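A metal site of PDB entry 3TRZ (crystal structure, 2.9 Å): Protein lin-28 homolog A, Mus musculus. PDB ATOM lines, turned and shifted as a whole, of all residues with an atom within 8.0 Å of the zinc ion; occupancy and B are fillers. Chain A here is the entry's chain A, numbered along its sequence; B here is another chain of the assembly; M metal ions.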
ATOM      1  N   VAL A  85     -10.991 -22.777   0.076  1.00  0.00           N
ATOM      2  CA  VAL A  85     -11.540 -22.880  -1.272  1.00  0.00           C
ATOM      3  C   VAL A  85     -12.687 -23.915  -1.235  1.00  0.00           C
ATOM      4  O   VAL A  85     -12.765 -24.721  -0.310  1.00  0.00           O
ATOM      5  CB  VAL A  85     -10.346 -23.311  -2.167  1.00  0.00           C
ATOM      6  CG1 VAL A  85     -10.760 -24.100  -3.387  1.00  0.00           C
ATOM      7  CG2 VAL A  85      -9.510 -22.096  -2.575  1.00  0.00           C
ATOM      8  N   PHE A  86     -13.597 -23.852  -2.214  1.00  0.00           N
ATOM      9  CA  PHE A  86     -14.705 -24.796  -2.270  1.00  0.00           C
ATOM     10  C   PHE A  86     -14.219 -26.221  -2.549  1.00  0.00           C
ATOM     11  O   PHE A  86     -13.185 -26.386  -3.194  1.00  0.00           O
ATOM     12  CB  PHE A  86     -15.668 -24.369  -3.388  1.00  0.00           C
ATOM     13  CG  PHE A  86     -16.284 -23.012  -3.187  1.00  0.00           C
ATOM     14  CD1 PHE A  86     -17.110 -22.761  -2.100  1.00  0.00           C
ATOM     15  CD2 PHE A  86     -16.110 -22.011  -4.132  1.00  0.00           C
ATOM     16  CE1 PHE A  86     -17.723 -21.518  -1.951  1.00  0.00           C
ATOM     17  CE2 PHE A  86     -16.740 -20.767  -3.972  1.00  0.00           C
ATOM     18  CZ  PHE A  86     -17.549 -20.539  -2.895  1.00  0.00           C
ATOM     19  N   ARG A  99     -15.408 -24.202 -12.987  1.00  0.00           N
ATOM     20  CA  ARG A  99     -14.946 -23.520 -11.783  1.00  0.00           C
ATOM     21  C   ARG A  99     -13.619 -22.799 -11.842  1.00  0.00           C
ATOM     22  O   ARG A  99     -12.693 -23.272 -12.483  1.00  0.00           O
ATOM     23  CB  ARG A  99     -15.045 -24.430 -10.558  1.00  0.00           C
ATOM     24  CG  ARG A  99     -14.458 -25.817 -10.709  1.00  0.00           C
ATOM     25  CD  ARG A  99     -13.855 -26.333  -9.411  1.00  0.00           C
ATOM     26  NE  ARG A  99     -14.846 -26.346  -8.340  1.00  0.00           N
ATOM     27  CZ  ARG A  99     -14.578 -26.432  -7.049  1.00  0.00           C
ATOM     28  NH1 ARG A  99     -13.316 -26.513  -6.629  1.00  0.00           N
ATOM     29  NH2 ARG A  99     -15.559 -26.400  -6.157  1.00  0.00           N
ATOM     30  N   CYS A 100     -13.531 -21.642 -11.140  1.00  0.00           N
ATOM     31  CA  CYS A 100     -12.364 -20.759 -11.003  1.00  0.00           C
ATOM     32  C   CYS A 100     -11.124 -21.514 -10.486  1.00  0.00           C
ATOM     33  O   CYS A 100     -11.225 -22.273  -9.523  1.00  0.00           O
ATOM     34  CB  CYS A 100     -12.715 -19.578 -10.101  1.00  0.00           C
ATOM     35  SG  CYS A 100     -11.320 -18.484  -9.704  1.00  0.00           S
ATOM     36  N   TYR A 101      -9.969 -21.298 -11.133  1.00  0.00           N
ATOM     37  CA  TYR A 101      -8.711 -21.939 -10.724  1.00  0.00           C
ATOM     38  C   TYR A 101      -8.183 -21.358  -9.406  1.00  0.00           C
ATOM     39  O   TYR A 101      -7.366 -21.997  -8.744  1.00  0.00           O
ATOM     40  CB  TYR A 101      -7.633 -21.829 -11.829  1.00  0.00           C
ATOM     41  CG  TYR A 101      -7.897 -22.632 -13.090  1.00  0.00           C
ATOM     42  CD1 TYR A 101      -8.507 -23.878 -13.025  1.00  0.00           C
ATOM     43  CD2 TYR A 101      -7.456 -22.184 -14.333  1.00  0.00           C
ATOM     44  CE1 TYR A 101      -8.767 -24.621 -14.182  1.00  0.00           C
ATOM     45  CE2 TYR A 101      -7.693 -22.923 -15.492  1.00  0.00           C
ATOM     46  CZ  TYR A 101      -8.362 -24.141 -15.409  1.00  0.00           C
ATOM     47  OH  TYR A 101      -8.616 -24.893 -16.537  1.00  0.00           O
ATOM     48  N   ASN A 102      -8.626 -20.159  -9.029  1.00  0.00           N
ATOM     49  CA  ASN A 102      -8.200 -19.526  -7.787  1.00  0.00           C
ATOM     50  C   ASN A 102      -9.062 -19.889  -6.566  1.00  0.00           C
ATOM     51  O   ASN A 102      -8.510 -20.105  -5.499  1.00  0.00           O
ATOM     52  CB  ASN A 102      -8.083 -18.009  -7.944  1.00  0.00           C
ATOM     53  CG  ASN A 102      -7.308 -17.383  -6.816  1.00  0.00           C
ATOM     54  OD1 ASN A 102      -6.118 -17.623  -6.651  1.00  0.00           O
ATOM     55  ND2 ASN A 102      -7.976 -16.571  -6.025  1.00  0.00           N
ATOM     56  N   CYS A 103     -10.389 -19.962  -6.720  1.00  0.00           N
ATOM     57  CA  CYS A 103     -11.270 -20.206  -5.574  1.00  0.00           C
ATOM     58  C   CYS A 103     -12.231 -21.414  -5.649  1.00  0.00           C
ATOM     59  O   CYS A 103     -12.818 -21.778  -4.634  1.00  0.00           O
ATOM     60  CB  CYS A 103     -12.043 -18.922  -5.246  1.00  0.00           C
ATOM     61  SG  CYS A 103     -13.257 -18.458  -6.511  1.00  0.00           S
ATOM     62  N   GLY A 104     -12.416 -21.952  -6.844  1.00  0.00           N
ATOM     63  CA  GLY A 104     -13.329 -23.061  -7.076  1.00  0.00           C
ATOM     64  C   GLY A 104     -14.750 -22.622  -7.342  1.00  0.00           C
ATOM     65  O   GLY A 104     -15.636 -23.465  -7.476  1.00  0.00           O
ATOM     66  N   GLY A 105     -14.972 -21.304  -7.396  1.00  0.00           N
ATOM     67  CA  GLY A 105     -16.279 -20.704  -7.671  1.00  0.00           C
ATOM     68  C   GLY A 105     -16.774 -21.024  -9.077  1.00  0.00           C
ATOM     69  O   GLY A 105     -15.964 -21.114 -10.002  1.00  0.00           O
ATOM     70  N   LEU A 106     -18.111 -21.218  -9.244  1.00  0.00           N
ATOM     71  CA  LEU A 106     -18.694 -21.579 -10.544  1.00  0.00           C
ATOM     72  C   LEU A 106     -18.985 -20.416 -11.491  1.00  0.00           C
ATOM     73  O   LEU A 106     -18.974 -20.602 -12.717  1.00  0.00           O
ATOM     74  CB  LEU A 106     -19.943 -22.472 -10.387  1.00  0.00           C
ATOM     75  CG  LEU A 106     -19.818 -23.749  -9.520  1.00  0.00           C
ATOM     76  CD1 LEU A 106     -21.191 -24.306  -9.151  1.00  0.00           C
ATOM     77  CD2 LEU A 106     -18.973 -24.840 -10.182  1.00  0.00           C
ATOM     78  N   ASP A 107     -19.222 -19.221 -10.944  1.00  0.00           N
ATOM     79  CA  ASP A 107     -19.600 -18.027 -11.726  1.00  0.00           C
ATOM     80  C   ASP A 107     -18.544 -17.375 -12.648  1.00  0.00           C
ATOM     81  O   ASP A 107     -18.923 -16.604 -13.538  1.00  0.00           O
ATOM     82  CB  ASP A 107     -20.155 -16.943 -10.773  1.00  0.00           C
ATOM     83  CG  ASP A 107     -21.414 -17.330 -10.023  1.00  0.00           C
ATOM     84  OD1 ASP A 107     -22.536 -17.087 -10.562  1.00  0.00           O
ATOM     85  OD2 ASP A 107     -21.281 -17.903  -8.907  1.00  0.00           O
ATOM     86  N   HIS A 108     -17.241 -17.609 -12.409  1.00  0.00           N
ATOM     87  CA  HIS A 108     -16.174 -16.894 -13.100  1.00  0.00           C
ATOM     88  C   HIS A 108     -14.878 -17.696 -13.287  1.00  0.00           C
ATOM     89  O   HIS A 108     -14.793 -18.873 -12.920  1.00  0.00           O
ATOM     90  CB  HIS A 108     -15.835 -15.626 -12.273  1.00  0.00           C
ATOM     91  CG  HIS A 108     -15.299 -15.943 -10.898  1.00  0.00           C
ATOM     92  ND1 HIS A 108     -16.109 -16.504  -9.917  1.00  0.00           N
ATOM     93  CD2 HIS A 108     -14.034 -15.862 -10.420  1.00  0.00           C
ATOM     94  CE1 HIS A 108     -15.320 -16.709  -8.883  1.00  0.00           C
ATOM     95  NE2 HIS A 108     -14.064 -16.341  -9.131  1.00  0.00           N
ATOM     96  N   HIS A 109     -13.857 -17.009 -13.839  1.00  0.00           N
ATOM     97  CA  HIS A 109     -12.510 -17.518 -14.106  1.00  0.00           C
ATOM     98  C   HIS A 109     -11.468 -16.722 -13.298  1.00  0.00           C
ATOM     99  O   HIS A 109     -11.741 -15.572 -12.927  1.00  0.00           O
ATOM    100  CB  HIS A 109     -12.184 -17.457 -15.610  1.00  0.00           C
ATOM    101  CG  HIS A 109     -12.862 -18.500 -16.446  1.00  0.00           C
ATOM    102  ND1 HIS A 109     -12.938 -18.372 -17.826  1.00  0.00           N
ATOM    103  CD2 HIS A 109     -13.488 -19.644 -16.078  1.00  0.00           C
ATOM    104  CE1 HIS A 109     -13.603 -19.437 -18.249  1.00  0.00           C
ATOM    105  NE2 HIS A 109     -13.943 -20.235 -17.235  1.00  0.00           N
ATOM    106  N   ALA A 110     -10.277 -17.336 -13.062  1.00  0.00           N
ATOM    107  CA  ALA A 110      -9.164 -16.786 -12.265  1.00  0.00           C
ATOM    108  C   ALA A 110      -8.784 -15.317 -12.526  1.00  0.00           C
ATOM    109  O   ALA A 110      -8.395 -14.637 -11.581  1.00  0.00           O
ATOM    110  CB  ALA A 110      -7.953 -17.681 -12.358  1.00  0.00           C
ATOM    111  N   LYS A 111      -8.923 -14.846 -13.787  1.00  0.00           N
ATOM    112  CA  LYS A 111      -8.609 -13.470 -14.215  1.00  0.00           C
ATOM    113  C   LYS A 111      -9.542 -12.451 -13.561  1.00  0.00           C
ATOM    114  O   LYS A 111      -9.092 -11.356 -13.225  1.00  0.00           O
ATOM    115  CB  LYS A 111      -8.705 -13.336 -15.745  1.00  0.00           C
ATOM    116  CG  LYS A 111      -7.863 -14.314 -16.553  1.00  0.00           C
ATOM    117  CD  LYS A 111      -8.371 -14.335 -17.989  1.00  0.00           C
ATOM    118  CE  LYS A 111      -7.653 -15.358 -18.827  1.00  0.00           C
ATOM    119  NZ  LYS A 111      -8.004 -15.231 -20.277  1.00  0.00           N
ATOM    120  N   GLU A 112     -10.831 -12.803 -13.409  1.00  0.00           N
ATOM    121  CA  GLU A 112     -11.874 -11.951 -12.837  1.00  0.00           C
ATOM    122  C   GLU A 112     -12.111 -12.196 -11.315  1.00  0.00           C
ATOM    123  O   GLU A 112     -12.968 -11.523 -10.720  1.00  0.00           O
ATOM    124  CB  GLU A 112     -13.211 -12.128 -13.608  1.00  0.00           C
ATOM    125  CG  GLU A 112     -13.103 -12.241 -15.123  1.00  0.00           C
ATOM    126  CD  GLU A 112     -13.571 -13.570 -15.715  1.00  0.00           C
ATOM    127  OE1 GLU A 112     -14.606 -14.098 -15.251  1.00  0.00           O
ATOM    128  OE2 GLU A 112     -12.926 -14.045 -16.672  1.00  0.00           O
ATOM    129  N   CYS A 113     -11.357 -13.139 -10.691  1.00  0.00           N
ATOM    130  CA  CYS A 113     -11.516 -13.490  -9.269  1.00  0.00           C
ATOM    131  C   CYS A 113     -11.273 -12.318  -8.327  1.00  0.00           C
ATOM    132  O   CYS A 113     -10.237 -11.646  -8.404  1.00  0.00           O
ATOM    133  CB  CYS A 113     -10.648 -14.699  -8.895  1.00  0.00           C
ATOM    134  SG  CYS A 113     -11.144 -15.525  -7.361  1.00  0.00           S
ATOM    135  N   LYS A 114     -12.266 -12.050  -7.480  1.00  0.00           N
ATOM    136  CA  LYS A 114     -12.236 -10.949  -6.523  1.00  0.00           C
ATOM    137  C   LYS A 114     -11.510 -11.317  -5.218  1.00  0.00           C
ATOM    138  O   LYS A 114     -11.162 -10.435  -4.425  1.00  0.00           O
ATOM    139  CB  LYS A 114     -13.666 -10.439  -6.259  1.00  0.00           C
ATOM    140  CG  LYS A 114     -14.229  -9.594  -7.401  1.00  0.00           C
ATOM    141  CD  LYS A 114     -15.745  -9.483  -7.368  1.00  0.00           C
ATOM    142  CE  LYS A 114     -16.281  -8.837  -8.615  1.00  0.00           C
ATOM    143  NZ  LYS A 114     -17.765  -8.911  -8.660  1.00  0.00           N
ATOM    144  N   LEU A 115     -11.261 -12.619  -5.019  1.00  0.00           N
ATOM    145  CA  LEU A 115     -10.600 -13.151  -3.839  1.00  0.00           C
ATOM    146  C   LEU A 115      -9.073 -13.066  -3.918  1.00  0.00           C
ATOM    147  O   LEU A 115      -8.529 -12.986  -5.037  1.00  0.00           O
ATOM    148  CB  LEU A 115     -11.073 -14.557  -3.560  1.00  0.00           C
ATOM    149  CG  LEU A 115     -12.453 -14.607  -2.944  1.00  0.00           C
ATOM    150  CD1 LEU A 115     -13.151 -15.898  -3.299  1.00  0.00           C
ATOM    151  CD2 LEU A 115     -12.390 -14.410  -1.438  1.00  0.00           C
ATOM    152  N   PRO A 116      -8.344 -13.012  -2.756  1.00  0.00           N
ATOM    153  CA  PRO A 116      -6.881 -12.882  -2.825  1.00  0.00           C
ATOM    154  C   PRO A 116      -6.234 -14.115  -3.464  1.00  0.00           C
ATOM    155  O   PRO A 116      -6.807 -15.212  -3.342  1.00  0.00           O
ATOM    156  CB  PRO A 116      -6.453 -12.682  -1.371  1.00  0.00           C
ATOM    157  CG  PRO A 116      -7.585 -13.171  -0.543  1.00  0.00           C
ATOM    158  CD  PRO A 116      -8.826 -13.049  -1.357  1.00  0.00           C
ATOM    159  P     G B  21      -5.807 -18.805 -20.657  1.00  0.00           P
ATOM    160  OP1   G B  21      -4.951 -19.584 -21.583  1.00  0.00           O
ATOM    161  OP2   G B  21      -5.978 -17.336 -20.808  1.00  0.00           O
ATOM    162  O5'   G B  21      -7.265 -19.487 -20.662  1.00  0.00           O
ATOM    163  C5'   G B  21      -7.852 -19.988 -21.847  1.00  0.00           C
ATOM    164  C4'   G B  21      -9.068 -20.838 -21.539  1.00  0.00           C
ATOM    165  O4'   G B  21      -8.891 -21.488 -20.270  1.00  0.00           O
ATOM    166  C3'   G B  21     -10.391 -20.087 -21.475  1.00  0.00           C
ATOM    167  O3'   G B  21     -11.030 -20.117 -22.760  1.00  0.00           O
ATOM    168  C2'   G B  21     -11.189 -20.885 -20.449  1.00  0.00           C
ATOM    169  O2'   G B  21     -12.020 -21.886 -21.034  1.00  0.00           O
ATOM    170  C1'   G B  21     -10.111 -21.500 -19.562  1.00  0.00           C
ATOM    171  N9    G B  21      -9.936 -20.892 -18.232  1.00  0.00           N
ATOM    172  C8    G B  21      -9.238 -19.749 -17.931  1.00  0.00           C
ATOM    173  N7    G B  21      -9.229 -19.446 -16.656  1.00  0.00           N
ATOM    174  C5    G B  21      -9.974 -20.450 -16.063  1.00  0.00           C
ATOM    175  C6    G B  21     -10.340 -20.654 -14.699  1.00  0.00           C
ATOM    176  O6    G B  21     -10.018 -19.960 -13.709  1.00  0.00           O
ATOM    177  N1    G B  21     -11.106 -21.812 -14.527  1.00  0.00           N
ATOM    178  C2    G B  21     -11.493 -22.659 -15.543  1.00  0.00           C
ATOM    179  N2    G B  21     -12.230 -23.723 -15.208  1.00  0.00           N
ATOM    180  N3    G B  21     -11.168 -22.471 -16.819  1.00  0.00           N
ATOM    181  C4    G B  21     -10.421 -21.354 -17.021  1.00  0.00           C
HETATM  182 ZN    ZN M   1     -12.421 -17.195  -8.071  1.00  0.00          ZN
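The zinc ion is bound by NE2 of His 108 (2.1 Å), SG of Cys 103 (2.2 Å), SG of Cys 113 (2.2 Å) and SG of Cys 100 (2.4 Å). The zinc ion has four donor atoms within binding distance.
The nearest printed residue that does not touch the zinc ion is Asn 102 (4.4 Å).
SG of Cys 103 lies close to N of Gly 105 (3.4 Å). The backbone carbonyl oxygen (O) of Cys 103 is in hydrogen-bond range of the backbone NH (N) of Phe 86 (3.3 Å). The side-chain sulfur (SG) of Cys 113 lies close to the side-chain amide nitrogen (ND2) of Asn 102, at 3.6 Å. The side-chain sulfur (SG) of Cys 113 lies close to the backbone NH (N) of Leu 115 (3.7 Å). The side-chain sulfur (SG) of Cys 100 sits close to the backbone NH (N) of Asn 102. N of Cys 100 sits at hydrogen-bond distance from O of Gly 105, 2.7 Å away. The side-chain sulfur (SG) of Cys 100 lies close to the backbone NH (N) of Ala 110, 3.7 Å away.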
